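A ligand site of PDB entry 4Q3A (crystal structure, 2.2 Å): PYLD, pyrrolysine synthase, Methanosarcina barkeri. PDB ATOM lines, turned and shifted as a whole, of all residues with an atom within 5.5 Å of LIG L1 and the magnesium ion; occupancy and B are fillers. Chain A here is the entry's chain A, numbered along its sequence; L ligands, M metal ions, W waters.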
ATOM      1  N   ALA A   3     -21.111 -20.686  33.596  1.00  0.00           N
ATOM      2  CA  ALA A   3     -21.392 -20.099  32.283  1.00  0.00           C
ATOM      3  C   ALA A   3     -22.839 -20.317  31.832  1.00  0.00           C
ATOM      4  O   ALA A   3     -23.140 -21.280  31.095  1.00  0.00           O
ATOM      5  CB  ALA A   3     -20.425 -20.664  31.253  1.00  0.00           C
ATOM      6  N   LEU A   4     -23.713 -19.399  32.256  1.00  0.00           N
ATOM      7  CA  LEU A   4     -25.145 -19.475  31.919  1.00  0.00           C
ATOM      8  C   LEU A   4     -25.596 -18.472  30.856  1.00  0.00           C
ATOM      9  O   LEU A   4     -25.135 -17.326  30.821  1.00  0.00           O
ATOM     10  CB  LEU A   4     -25.999 -19.262  33.174  1.00  0.00           C
ATOM     11  CG  LEU A   4     -25.716 -20.189  34.370  1.00  0.00           C
ATOM     12  CD1 LEU A   4     -26.772 -19.969  35.419  1.00  0.00           C
ATOM     13  CD2 LEU A   4     -25.675 -21.651  33.955  1.00  0.00           C
ATOM     14  N   ASN A 122     -27.214 -32.420  28.308  1.00  0.00           N
ATOM     15  CA  ASN A 122     -26.790 -31.424  27.341  1.00  0.00           C
ATOM     16  C   ASN A 122     -25.274 -31.335  27.082  1.00  0.00           C
ATOM     17  O   ASN A 122     -24.847 -31.058  25.951  1.00  0.00           O
ATOM     18  CB  ASN A 122     -27.320 -30.054  27.779  1.00  0.00           C
ATOM     19  CG  ASN A 122     -26.924 -28.933  26.842  1.00  0.00           C
ATOM     20  OD1 ASN A 122     -26.065 -28.112  27.177  1.00  0.00           O
ATOM     21  ND2 ASN A 122     -27.540 -28.891  25.679  1.00  0.00           N
ATOM     22  N   GLN A 123     -24.473 -31.531  28.122  1.00  0.00           N
ATOM     23  CA  GLN A 123     -23.029 -31.301  28.000  1.00  0.00           C
ATOM     24  C   GLN A 123     -22.350 -32.313  27.055  1.00  0.00           C
ATOM     25  O   GLN A 123     -21.752 -31.912  26.070  1.00  0.00           O
ATOM     26  CB  GLN A 123     -22.372 -31.223  29.390  1.00  0.00           C
ATOM     27  CG  GLN A 123     -22.777 -29.939  30.091  1.00  0.00           C
ATOM     28  CD  GLN A 123     -22.571 -29.920  31.602  1.00  0.00           C
ATOM     29  OE1 GLN A 123     -22.416 -28.850  32.208  1.00  0.00           O
ATOM     30  NE2 GLN A 123     -22.570 -31.071  32.222  1.00  0.00           N
ATOM     31  N   THR A 126     -23.937 -31.890  23.422  1.00  0.00           N
ATOM     32  CA  THR A 126     -23.390 -30.738  22.741  1.00  0.00           C
ATOM     33  C   THR A 126     -21.970 -30.971  22.235  1.00  0.00           C
ATOM     34  O   THR A 126     -21.655 -30.659  21.091  1.00  0.00           O
ATOM     35  CB  THR A 126     -23.432 -29.499  23.653  1.00  0.00           C
ATOM     36  OG1 THR A 126     -24.811 -29.248  24.013  1.00  0.00           O
ATOM     37  CG2 THR A 126     -22.816 -28.320  22.945  1.00  0.00           C
ATOM     38  N   TYR A 130     -21.150 -31.017  17.953  1.00  0.00           N
ATOM     39  CA  TYR A 130     -20.223 -30.055  17.386  1.00  0.00           C
ATOM     40  C   TYR A 130     -18.911 -30.715  16.947  1.00  0.00           C
ATOM     41  O   TYR A 130     -18.271 -30.243  16.010  1.00  0.00           O
ATOM     42  CB  TYR A 130     -19.927 -28.896  18.354  1.00  0.00           C
ATOM     43  CG  TYR A 130     -20.988 -27.820  18.402  1.00  0.00           C
ATOM     44  CD1 TYR A 130     -22.085 -27.933  19.251  1.00  0.00           C
ATOM     45  CD2 TYR A 130     -20.890 -26.668  17.632  1.00  0.00           C
ATOM     46  CE1 TYR A 130     -23.055 -26.931  19.328  1.00  0.00           C
ATOM     47  CE2 TYR A 130     -21.852 -25.663  17.699  1.00  0.00           C
ATOM     48  CZ  TYR A 130     -22.941 -25.807  18.540  1.00  0.00           C
ATOM     49  OH  TYR A 130     -23.913 -24.814  18.611  1.00  0.00           O
ATOM     50  N   VAL A 148      -9.925 -27.049  21.791  1.00  0.00           N
ATOM     51  CA  VAL A 148      -9.584 -26.039  22.783  1.00  0.00           C
ATOM     52  C   VAL A 148     -10.690 -25.978  23.839  1.00  0.00           C
ATOM     53  O   VAL A 148     -11.810 -25.535  23.548  1.00  0.00           O
ATOM     54  CB  VAL A 148      -9.404 -24.652  22.129  1.00  0.00           C
ATOM     55  CG1 VAL A 148      -9.122 -23.569  23.170  1.00  0.00           C
ATOM     56  CG2 VAL A 148      -8.260 -24.687  21.119  1.00  0.00           C
ATOM     57  N   GLY A 149     -10.364 -26.410  25.050  1.00  0.00           N
ATOM     58  CA  GLY A 149     -11.359 -26.546  26.118  1.00  0.00           C
ATOM     59  C   GLY A 149     -11.720 -28.001  26.264  1.00  0.00           C
ATOM     60  O   GLY A 149     -12.323 -28.595  25.382  1.00  0.00           O
ATOM     61  N   LEU A 150     -11.353 -28.585  27.406  1.00  0.00           N
ATOM     62  CA  LEU A 150     -11.535 -30.009  27.655  1.00  0.00           C
ATOM     63  C   LEU A 150     -12.322 -30.232  28.928  1.00  0.00           C
ATOM     64  O   LEU A 150     -12.003 -31.105  29.732  1.00  0.00           O
ATOM     65  CB  LEU A 150     -10.160 -30.681  27.713  1.00  0.00           C
ATOM     66  CG  LEU A 150      -9.344 -30.589  26.419  1.00  0.00           C
ATOM     67  CD1 LEU A 150      -7.872 -30.904  26.640  1.00  0.00           C
ATOM     68  CD2 LEU A 150      -9.940 -31.498  25.375  1.00  0.00           C
ATOM     69  N   GLY A 151     -13.371 -29.429  29.107  1.00  0.00           N
ATOM     70  CA  GLY A 151     -14.248 -29.528  30.265  1.00  0.00           C
ATOM     71  C   GLY A 151     -15.431 -30.413  29.963  1.00  0.00           C
ATOM     72  O   GLY A 151     -15.331 -31.385  29.200  1.00  0.00           O
ATOM     73  N   LYS A 152     -16.571 -30.059  30.531  1.00  0.00           N
ATOM     74  CA  LYS A 152     -17.767 -30.883  30.453  1.00  0.00           C
ATOM     75  C   LYS A 152     -18.321 -31.063  29.050  1.00  0.00           C
ATOM     76  O   LYS A 152     -18.894 -32.112  28.759  1.00  0.00           O
ATOM     77  CB  LYS A 152     -18.827 -30.317  31.402  1.00  0.00           C
ATOM     78  CG  LYS A 152     -18.331 -30.338  32.846  1.00  0.00           C
ATOM     79  CD  LYS A 152     -19.445 -30.485  33.862  1.00  0.00           C
ATOM     80  CE  LYS A 152     -18.883 -30.897  35.222  1.00  0.00           C
ATOM     81  NZ  LYS A 152     -18.652 -29.701  36.079  1.00  0.00           N
ATOM     82  N   VAL A 153     -18.163 -30.059  28.198  1.00  0.00           N
ATOM     83  CA  VAL A 153     -18.558 -30.146  26.797  1.00  0.00           C
ATOM     84  C   VAL A 153     -17.376 -30.628  25.953  1.00  0.00           C
ATOM     85  O   VAL A 153     -17.534 -31.511  25.119  1.00  0.00           O
ATOM     86  CB  VAL A 153     -19.069 -28.777  26.269  1.00  0.00           C
ATOM     87  CG1 VAL A 153     -19.322 -28.788  24.779  1.00  0.00           C
ATOM     88  CG2 VAL A 153     -20.358 -28.388  26.977  1.00  0.00           C
ATOM     89  N   GLY A 154     -16.200 -30.063  26.208  1.00  0.00           N
ATOM     90  CA  GLY A 154     -15.008 -30.327  25.407  1.00  0.00           C
ATOM     91  C   GLY A 154     -14.461 -31.745  25.520  1.00  0.00           C
ATOM     92  O   GLY A 154     -14.036 -32.332  24.525  1.00  0.00           O
ATOM     93  N   TYR A 171      -5.919 -28.692  24.011  1.00  0.00           N
ATOM     94  CA  TYR A 171      -5.408 -27.666  24.911  1.00  0.00           C
ATOM     95  C   TYR A 171      -6.481 -27.203  25.883  1.00  0.00           C
ATOM     96  O   TYR A 171      -7.620 -27.005  25.499  1.00  0.00           O
ATOM     97  CB  TYR A 171      -4.905 -26.456  24.118  1.00  0.00           C
ATOM     98  CG  TYR A 171      -4.370 -25.392  25.026  1.00  0.00           C
ATOM     99  CD1 TYR A 171      -3.150 -25.555  25.677  1.00  0.00           C
ATOM    100  CD2 TYR A 171      -5.085 -24.223  25.253  1.00  0.00           C
ATOM    101  CE1 TYR A 171      -2.650 -24.580  26.526  1.00  0.00           C
ATOM    102  CE2 TYR A 171      -4.604 -23.237  26.110  1.00  0.00           C
ATOM    103  CZ  TYR A 171      -3.379 -23.431  26.731  1.00  0.00           C
ATOM    104  OH  TYR A 171      -2.871 -22.465  27.574  1.00  0.00           O
ATOM    105  N   ASP A 172      -6.092 -27.045  27.141  1.00  0.00           N
ATOM    106  CA  ASP A 172      -6.948 -26.397  28.138  1.00  0.00           C
ATOM    107  C   ASP A 172      -6.030 -25.540  28.987  1.00  0.00           C
ATOM    108  O   ASP A 172      -4.918 -25.960  29.280  1.00  0.00           O
ATOM    109  CB  ASP A 172      -7.674 -27.438  28.997  1.00  0.00           C
ATOM    110  CG  ASP A 172      -8.829 -26.856  29.780  1.00  0.00           C
ATOM    111  OD1 ASP A 172      -8.552 -26.067  30.709  1.00  0.00           O
ATOM    112  OD2 ASP A 172     -10.008 -27.185  29.477  1.00  0.00           O
ATOM    113  N   ALA A 173      -6.506 -24.352  29.384  1.00  0.00           N
ATOM    114  CA  ALA A 173      -5.699 -23.460  30.220  1.00  0.00           C
ATOM    115  C   ALA A 173      -5.447 -24.026  31.606  1.00  0.00           C
ATOM    116  O   ALA A 173      -4.495 -23.619  32.259  1.00  0.00           O
ATOM    117  CB  ALA A 173      -6.349 -22.091  30.323  1.00  0.00           C
ATOM    118  N   ASP A 174      -6.316 -24.938  32.068  1.00  0.00           N
ATOM    119  CA  ASP A 174      -6.087 -25.683  33.306  1.00  0.00           C
ATOM    120  C   ASP A 174      -5.261 -26.935  32.972  1.00  0.00           C
ATOM    121  O   ASP A 174      -5.717 -27.826  32.248  1.00  0.00           O
ATOM    122  CB  ASP A 174      -7.425 -26.077  33.936  1.00  0.00           C
ATOM    123  CG  ASP A 174      -7.276 -26.919  35.220  1.00  0.00           C
ATOM    124  OD1 ASP A 174      -6.214 -27.535  35.462  1.00  0.00           O
ATOM    125  OD2 ASP A 174      -8.235 -26.956  36.004  1.00  0.00           O
ATOM    126  N   LEU A 177      -6.788 -30.392  33.804  1.00  0.00           N
ATOM    127  CA  LEU A 177      -7.754 -30.856  32.805  1.00  0.00           C
ATOM    128  C   LEU A 177      -7.017 -31.395  31.583  1.00  0.00           C
ATOM    129  O   LEU A 177      -7.395 -32.431  31.034  1.00  0.00           O
ATOM    130  CB  LEU A 177      -8.732 -29.743  32.378  1.00  0.00           C
ATOM    131  CG  LEU A 177     -10.083 -29.589  33.108  1.00  0.00           C
ATOM    132  CD1 LEU A 177     -10.849 -30.905  33.195  1.00  0.00           C
ATOM    133  CD2 LEU A 177      -9.902 -29.010  34.495  1.00  0.00           C
ATOM    134  N   ALA A 204     -14.617 -25.236  23.004  1.00  0.00           N
ATOM    135  CA  ALA A 204     -15.642 -25.286  24.032  1.00  0.00           C
ATOM    136  C   ALA A 204     -15.187 -24.609  25.317  1.00  0.00           C
ATOM    137  O   ALA A 204     -15.005 -25.273  26.340  1.00  0.00           O
ATOM    138  CB  ALA A 204     -16.056 -26.731  24.295  1.00  0.00           C
ATOM    139  N   THR A 205     -15.032 -23.284  25.269  1.00  0.00           N
ATOM    140  CA  THR A 205     -14.723 -22.480  26.470  1.00  0.00           C
ATOM    141  C   THR A 205     -15.730 -21.335  26.588  1.00  0.00           C
ATOM    142  O   THR A 205     -16.351 -20.956  25.588  1.00  0.00           O
ATOM    143  CB  THR A 205     -13.311 -21.836  26.443  1.00  0.00           C
ATOM    144  OG1 THR A 205     -13.344 -20.591  25.706  1.00  0.00           O
ATOM    145  CG2 THR A 205     -12.261 -22.761  25.843  1.00  0.00           C
ATOM    146  N   PRO A 206     -15.860 -20.743  27.785  1.00  0.00           N
ATOM    147  CA  PRO A 206     -16.704 -19.571  27.958  1.00  0.00           C
ATOM    148  C   PRO A 206     -15.962 -18.249  27.703  1.00  0.00           C
ATOM    149  O   PRO A 206     -16.391 -17.209  28.206  1.00  0.00           O
ATOM    150  CB  PRO A 206     -17.131 -19.682  29.430  1.00  0.00           C
ATOM    151  CG  PRO A 206     -15.955 -20.302  30.099  1.00  0.00           C
ATOM    152  CD  PRO A 206     -15.271 -21.170  29.063  1.00  0.00           C
ATOM    153  N   CYS A 207     -14.873 -18.288  26.941  1.00  0.00           N
ATOM    154  CA  CYS A 207     -14.007 -17.123  26.767  1.00  0.00           C
ATOM    155  C   CYS A 207     -13.843 -16.716  25.311  1.00  0.00           C
ATOM    156  O   CYS A 207     -13.867 -17.555  24.406  1.00  0.00           O
ATOM    157  CB  CYS A 207     -12.629 -17.420  27.368  1.00  0.00           C
ATOM    158  SG  CYS A 207     -12.641 -17.381  29.184  1.00  0.00           S
ATOM    159  N   THR A 210      -9.870 -17.311  22.028  1.00  0.00           N
ATOM    160  CA  THR A 210      -9.099 -18.444  22.502  1.00  0.00           C
ATOM    161  C   THR A 210      -8.315 -19.131  21.386  1.00  0.00           C
ATOM    162  O   THR A 210      -7.423 -19.934  21.654  1.00  0.00           O
ATOM    163  CB  THR A 210     -10.037 -19.469  23.162  1.00  0.00           C
ATOM    164  OG1 THR A 210     -11.050 -19.857  22.224  1.00  0.00           O
ATOM    165  CG2 THR A 210     -10.689 -18.879  24.393  1.00  0.00           C
ATOM    166  N   THR A 224     -17.947 -24.425  17.293  1.00  0.00           N
ATOM    167  CA  THR A 224     -17.868 -24.014  18.675  1.00  0.00           C
ATOM    168  C   THR A 224     -19.205 -23.762  19.391  1.00  0.00           C
ATOM    169  O   THR A 224     -19.965 -22.859  19.014  1.00  0.00           O
ATOM    170  CB  THR A 224     -16.907 -22.806  18.852  1.00  0.00           C
ATOM    171  OG1 THR A 224     -16.871 -22.424  20.233  1.00  0.00           O
ATOM    172  CG2 THR A 224     -17.306 -21.611  17.989  1.00  0.00           C
ATOM    173  N   PRO A 225     -19.494 -24.556  20.438  1.00  0.00           N
ATOM    174  CA  PRO A 225     -20.621 -24.251  21.313  1.00  0.00           C
ATOM    175  C   PRO A 225     -20.304 -23.149  22.314  1.00  0.00           C
ATOM    176  O   PRO A 225     -21.213 -22.593  22.915  1.00  0.00           O
ATOM    177  CB  PRO A 225     -20.887 -25.550  22.039  1.00  0.00           C
ATOM    178  CG  PRO A 225     -19.557 -26.223  22.067  1.00  0.00           C
ATOM    179  CD  PRO A 225     -18.907 -25.871  20.768  1.00  0.00           C
ATOM    180  N   GLY A 226     -19.017 -22.829  22.460  1.00  0.00           N
ATOM    181  CA  GLY A 226     -18.570 -21.810  23.411  1.00  0.00           C
ATOM    182  C   GLY A 226     -19.213 -20.440  23.223  1.00  0.00           C
ATOM    183  O   GLY A 226     -19.474 -20.013  22.106  1.00  0.00           O
ATOM    184  N   ILE A 227     -19.441 -19.765  24.340  1.00  0.00           N
ATOM    185  CA  ILE A 227     -20.076 -18.448  24.365  1.00  0.00           C
ATOM    186  C   ILE A 227     -19.290 -17.543  25.327  1.00  0.00           C
ATOM    187  O   ILE A 227     -19.015 -17.945  26.457  1.00  0.00           O
ATOM    188  CB  ILE A 227     -21.549 -18.556  24.852  1.00  0.00           C
ATOM    189  CG1 ILE A 227     -22.357 -19.531  23.979  1.00  0.00           C
ATOM    190  CG2 ILE A 227     -22.215 -17.185  24.853  1.00  0.00           C
ATOM    191  CD1 ILE A 227     -23.629 -20.047  24.624  1.00  0.00           C
ATOM    192  N   GLU A 246     -23.757 -21.539  17.758  1.00  0.00           N
ATOM    193  CA  GLU A 246     -25.166 -21.338  18.010  1.00  0.00           C
ATOM    194  C   GLU A 246     -25.417 -21.685  19.464  1.00  0.00           C
ATOM    195  O   GLU A 246     -24.875 -22.665  19.972  1.00  0.00           O
ATOM    196  CB  GLU A 246     -25.963 -22.205  17.025  1.00  0.00           C
ATOM    197  CG  GLU A 246     -27.472 -22.018  17.083  1.00  0.00           C
ATOM    198  CD  GLU A 246     -28.065 -22.761  18.240  1.00  0.00           C
ATOM    199  OE1 GLU A 246     -29.109 -22.301  18.800  1.00  0.00           O
ATOM    200  OE2 GLU A 246     -27.454 -23.798  18.626  1.00  0.00           O
ATOM    201  N   PRO A 247     -26.227 -20.884  20.161  1.00  0.00           N
ATOM    202  CA  PRO A 247     -26.253 -20.929  21.638  1.00  0.00           C
ATOM    203  C   PRO A 247     -27.037 -22.039  22.347  1.00  0.00           C
ATOM    204  O   PRO A 247     -26.839 -22.229  23.552  1.00  0.00           O
ATOM    205  CB  PRO A 247     -26.832 -19.567  22.020  1.00  0.00           C
ATOM    206  CG  PRO A 247     -27.680 -19.177  20.855  1.00  0.00           C
ATOM    207  CD  PRO A 247     -27.003 -19.735  19.640  1.00  0.00           C
ATOM    208  N   LEU A 248     -27.897 -22.786  21.637  1.00  0.00           N
ATOM    209  CA  LEU A 248     -28.773 -23.741  22.342  1.00  0.00           C
ATOM    210  C   LEU A 248     -29.404 -24.837  21.473  1.00  0.00           C
ATOM    211  O   LEU A 248     -29.557 -25.968  21.935  1.00  0.00           O
ATOM    212  CB  LEU A 248     -29.895 -22.965  23.060  1.00  0.00           C
ATOM    213  CG  LEU A 248     -30.893 -23.715  23.945  1.00  0.00           C
ATOM    214  CD1 LEU A 248     -30.219 -24.372  25.137  1.00  0.00           C
ATOM    215  CD2 LEU A 248     -32.012 -22.787  24.414  1.00  0.00           C
ATOM    216  N   GLY A 249     -29.790 -24.498  20.237  1.00  0.00           N
ATOM    217  CA  GLY A 249     -30.570 -25.377  19.371  1.00  0.00           C
ATOM    218  C   GLY A 249     -29.893 -26.644  18.858  1.00  0.00           C
ATOM    219  O   GLY A 249     -30.533 -27.688  18.799  1.00  0.00           O
ATOM    220  N   ILE A 250     -28.616 -26.565  18.493  1.00  0.00           N
ATOM    221  CA  ILE A 250     -27.871 -27.730  17.986  1.00  0.00           C
ATOM    222  C   ILE A 250     -27.659 -28.768  19.090  1.00  0.00           C
ATOM    223  O   ILE A 250     -27.913 -29.966  18.897  1.00  0.00           O
ATOM    224  CB  ILE A 250     -26.532 -27.295  17.344  1.00  0.00           C
ATOM    225  CG1 ILE A 250     -26.811 -26.468  16.078  1.00  0.00           C
ATOM    226  CG2 ILE A 250     -25.679 -28.488  16.961  1.00  0.00           C
ATOM    227  CD1 ILE A 250     -25.556 -25.971  15.390  1.00  0.00           C
ATOM    228  N   GLY A 251     -27.235 -28.293  20.249  1.00  0.00           N
ATOM    229  CA  GLY A 251     -27.100 -29.124  21.436  1.00  0.00           C
ATOM    230  C   GLY A 251     -28.411 -29.748  21.872  1.00  0.00           C
ATOM    231  O   GLY A 251     -28.439 -30.923  22.236  1.00  0.00           O
ATOM    232  N   THR A 252     -29.487 -28.974  21.804  1.00  0.00           N
ATOM    233  CA  THR A 252     -30.805 -29.484  22.144  1.00  0.00           C
ATOM    234  C   THR A 252     -31.240 -30.570  21.165  1.00  0.00           C
ATOM    235  O   THR A 252     -31.791 -31.594  21.561  1.00  0.00           O
ATOM    236  CB  THR A 252     -31.847 -28.363  22.170  1.00  0.00           C
ATOM    237  OG1 THR A 252     -31.468 -27.391  23.159  1.00  0.00           O
ATOM    238  CG2 THR A 252     -33.239 -28.931  22.508  1.00  0.00           C
HETATM  239  P1  LIG L   1     -16.437 -26.053  31.687  1.00  0.00           P
HETATM  240  O1  LIG L   1     -16.159 -24.982  32.710  1.00  0.00           O
HETATM  241  O2  LIG L   1     -16.749 -27.471  32.082  1.00  0.00           O
HETATM  242  O3  LIG L   1     -15.198 -26.166  30.667  1.00  0.00           O
HETATM  243  C1  LIG L   1     -14.661 -25.041  29.995  1.00  0.00           C
HETATM  244  C2  LIG L   1     -13.175 -25.262  29.861  1.00  0.00           C
HETATM  245  O4  LIG L   1     -12.563 -24.253  29.067  1.00  0.00           O
HETATM  246  C3  LIG L   1     -12.486 -25.243  31.225  1.00  0.00           C
HETATM  247  O5  LIG L   1     -11.811 -26.481  31.439  1.00  0.00           O
HETATM  248  C4  LIG L   1     -11.465 -24.138  31.161  1.00  0.00           C
HETATM  249  O6  LIG L   1     -10.241 -24.521  31.788  1.00  0.00           O
HETATM  250  C5  LIG L   1     -11.295 -23.981  29.652  1.00  0.00           C
HETATM  251  N1  LIG L   1     -10.820 -22.644  29.296  1.00  0.00           N
HETATM  252  C6  LIG L   1     -11.253 -21.463  29.777  1.00  0.00           C
HETATM  253  N2  LIG L   1     -10.588 -20.446  29.201  1.00  0.00           N
HETATM  254  C7  LIG L   1      -9.705 -20.978  28.339  1.00  0.00           C
HETATM  255  C8  LIG L   1      -8.677 -20.480  27.420  1.00  0.00           C
HETATM  256  N3  LIG L   1      -8.482 -19.153  27.298  1.00  0.00           N
HETATM  257  N4  LIG L   1      -7.979 -21.374  26.692  1.00  0.00           N
HETATM  258  C9  LIG L   1      -8.186 -22.703  26.802  1.00  0.00           C
HETATM  259  N5  LIG L   1      -9.087 -23.228  27.632  1.00  0.00           N
HETATM  260  C10 LIG L   1      -9.866 -22.438  28.401  1.00  0.00           C
HETATM  261  O7  LIG L   1     -17.622 -25.492  30.775  1.00  0.00           O
HETATM  262  P2  LIG L   1     -18.510 -26.417  29.813  1.00  0.00           P
HETATM  263  O8  LIG L   1     -19.704 -26.941  30.514  1.00  0.00           O
HETATM  264  O9  LIG L   1     -17.587 -27.361  29.054  1.00  0.00           O
HETATM  265  O10 LIG L   1     -19.054 -25.276  28.818  1.00  0.00           O
HETATM  266  C11 LIG L   1     -18.205 -24.652  27.865  1.00  0.00           C
HETATM  267  C12 LIG L   1     -18.941 -23.526  27.150  1.00  0.00           C
HETATM  268  O11 LIG L   1     -19.975 -24.076  26.342  1.00  0.00           O
HETATM  269  C13 LIG L   1     -19.623 -22.527  28.077  1.00  0.00           C
HETATM  270  O12 LIG L   1     -19.435 -21.197  27.563  1.00  0.00           O
HETATM  271  C14 LIG L   1     -21.095 -22.897  28.004  1.00  0.00           C
HETATM  272  O13 LIG L   1     -21.967 -21.793  28.222  1.00  0.00           O
HETATM  273  C15 LIG L   1     -21.184 -23.340  26.558  1.00  0.00           C
HETATM  274  N6  LIG L   1     -22.274 -24.247  26.211  1.00  0.00           N
HETATM  275  C16 LIG L   1     -22.899 -24.030  25.047  1.00  0.00           C
HETATM  276  C17 LIG L   1     -23.927 -24.842  24.597  1.00  0.00           C
HETATM  277  C18 LIG L   1     -24.577 -24.573  23.245  1.00  0.00           C
HETATM  278  O14 LIG L   1     -25.552 -25.209  22.880  1.00  0.00           O
HETATM  279  N7  LIG L   1     -24.011 -23.706  22.407  1.00  0.00           N
HETATM  280  C19 LIG L   1     -24.365 -26.031  25.418  1.00  0.00           C
HETATM  281  C20 LIG L   1     -23.603 -26.180  26.652  1.00  0.00           C
HETATM  282  C21 LIG L   1     -22.596 -25.294  26.997  1.00  0.00           C
HETATM  283  O1  LG2 L   2     -35.864 -22.952  33.264  1.00  0.00           O
HETATM  284  C1  LG2 L   2     -35.088 -21.997  33.116  1.00  0.00           C
HETATM  285  O2  LG2 L   2     -35.486 -20.911  32.445  1.00  0.00           O
HETATM  286  C2  LG2 L   2     -33.691 -22.043  33.677  1.00  0.00           C
HETATM  287  N1  LG2 L   2     -33.648 -22.880  34.858  1.00  0.00           N
HETATM  288  C3  LG2 L   2     -32.724 -22.575  32.630  1.00  0.00           C
HETATM  289  C4  LG2 L   2     -31.307 -22.710  33.159  1.00  0.00           C
HETATM  290  C5  LG2 L   2     -30.361 -23.084  32.043  1.00  0.00           C
HETATM  291  C6  LG2 L   2     -28.904 -22.965  32.461  1.00  0.00           C
HETATM  292  N2  LG2 L   2     -27.991 -23.542  31.486  1.00  0.00           N
HETATM  293  C7  LG2 L   2     -27.377 -22.765  30.591  1.00  0.00           C
HETATM  294  O3  LG2 L   2     -27.540 -21.554  30.559  1.00  0.00           O
HETATM  295  C8  LG2 L   2     -26.463 -23.412  29.576  1.00  0.00           C
HETATM  296  C9  LG2 L   2     -27.169 -23.580  28.232  1.00  0.00           C
HETATM  297  C10 LG2 L   2     -26.252 -23.275  27.050  1.00  0.00           C
HETATM  298  C11 LG2 L   2     -27.689 -25.009  28.190  1.00  0.00           C
HETATM  299  C12 LG2 L   2     -26.830 -25.632  29.254  1.00  0.00           C
HETATM  300  N3  LG2 L   2     -26.153 -24.785  29.916  1.00  0.00           N
HETATM  301 MG    MG M   1     -26.102 -25.235  20.345  1.00  0.00          MG
HETATM  302  O   HOH W   1     -20.586 -19.021  28.740  1.00  0.00           O
HETATM  303  O   HOH W   2     -27.419 -26.737  23.828  1.00  0.00           O
HETATM  304  O   HOH W   3     -14.822 -28.826  33.959  1.00  0.00           O
HETATM  305  O   HOH W   4     -13.489 -21.560  32.426  1.00  0.00           O
HETATM  306  O   HOH W   5     -10.445 -19.125  31.803  1.00  0.00           O
HETATM  307  O   HOH W   6     -15.403 -27.694  27.731  1.00  0.00           O
HETATM  308  O   HOH W   7     -22.352 -26.475  30.084  1.00  0.00           O
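The side-chain carboxylate of Asp 172 lies within hydrogen-bond range of an oxygen (O6) of LIG L1 (2.5 Å).
O of Glu 246 sits at hydrogen-bond distance from N7 of LIG L1, at 2.8 Å.
The backbone NH of Val 153 lies within hydrogen-bond range of an oxygen (O9) of LIG L1, 2.9 Å away.
The backbone NH (N) of Lys 152 lies within hydrogen-bond range of an oxygen (O2) of LIG L1 (3.0 Å).
N7 of LIG L1 lies within hydrogen-bond range of O of Pro 225.
The backbone carbonyl oxygen (O) of Ala 3 is in hydrogen-bond range of an oxygen (O13) of LIG L1, at 3.1 Å.
The backbone carbonyl oxygen (O) of Pro 247 sits close to a nitrogen (N7) of LIG L1, at 3.4 Å.
The backbone NH (N) of Ala 173 is in hydrogen-bond range of a nitrogen (N5) of LIG L1 (3.3 Å).
An oxygen (O12) of LIG L1 is in hydrogen-bond range of the backbone carbonyl oxygen of Ile 227 (3.5 Å).
N2 of LIG L1 lies within hydrogen-bond range of SG of Cys 207 (3.7 Å).
OD1 of Asp 172 is in hydrogen-bond range of N of Asp 174 (2.8 Å).
N of Leu 150 is in hydrogen-bond range of OD2 of Asp 172, at 2.8 Å.
The side-chain hydroxyl of Tyr 130 is in hydrogen-bond range of the backbone carbonyl oxygen of Glu 246, 2.7 Å away.
The backbone NH of Ile 250 sits at hydrogen-bond distance from the side-chain carboxylate of Glu 246 (3.0 Å).
The backbone NH of Gly 249 lies within hydrogen-bond range of the side-chain carboxylate of Glu 246 (2.7 Å).
OG1 of Thr 252 is in hydrogen-bond range of O of Leu 248, at 2.7 Å.
The side-chain hydroxyl (OG1) of Thr 205 lies within hydrogen-bond range of the backbone NH (N) of Cys 207, at 3.0 Å.
O of Tyr 171 is in hydrogen-bond range of N of Gly 149, at 2.8 Å.
Residues that only touch LIG L1: Asn 122 (3.2 Å), Gln 123 (3.7 Å), Thr 126 (3.5 Å), Val 148 (3.8 Å), Gly 149 (3.9 Å), Gly 151 (3.5 Å), Tyr 171 (3.7 Å), Asp 174 (3.9 Å), Leu 177 (3.9 Å), Ala 204 (3.6 Å), Thr 205 (3.5 Å), Pro 206 (3.2 Å), Thr 210 (3.7 Å), Gly 226 (3.96 Å) and Leu 248 (3.6 Å).
Hydrophobic or aromatic side chains within 4 Å of LIG L1: Ala 3, Val 148, Val 153, Tyr 171, Leu 177, Pro 206 and Pro 225.
Within 4 Å of LIG L1: Ala 3, Asn 122, Gln 123, Thr 126, Tyr 130, Val 148, Gly 149, Gly 151, Lys 152, Val 153, Tyr 171, Asp 172, Ala 173, Asp 174, Leu 177, Ala 204, Thr 205, Pro 206, Cys 207, Thr 210, Pro 225, Gly 226, Ile 227, Glu 246, Pro 247 and Leu 248.
Pro 247 touches the magnesium ion.
N of Leu 248 touches the magnesium ion (3.3 Å).
Gly 249 touches the magnesium ion.
Ile 250 touches the magnesium ion (N to MG, 3.4 Å).
Gly 251 touches the magnesium ion.
Of the 34 residues printed, 7 come within 4 Å of the magnesium ion.
Along chain A the residues within 4 Å of the magnesium ion span positions 130 to 251.
The nearest printed residue that does not touch the magnesium ion is Thr 126 (5.2 Å).
An oxygen (O14) of LIG L1 binds the magnesium ion, 2.6 Å away.
The magnesium ion has one donor atom within binding distance.
Slightly farther from the magnesium ion lies OE2 of Glu 246 (2.6 Å).
Slightly farther from the magnesium ion lies the side-chain hydroxyl (OH) of Tyr 130 (2.8 Å).
Water W6 lies within hydrogen-bond range of an oxygen (O9) of LIG L1 (2.6 Å), the backbone carbonyl oxygen (O) of Ala 204 (2.8 Å), the backbone NH (N) of Gly 154 (2.9 Å) and the backbone NH (N) of Gly 151 (3.0 Å).
Water W2 bridges ND2 of Asn 122 (2.8 Å) and O of Leu 248 (3.0 Å).
Water W7 bridges an oxygen (O8) of LIG L1 (2.7 Å) and the side-chain amide oxygen (OE1) of Gln 123 (3.2 Å).
Water W1 lies within hydrogen-bond range of an oxygen (O12) of LIG L1 (2.7 Å) and the backbone carbonyl oxygen of Ile 227 (3.0 Å).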
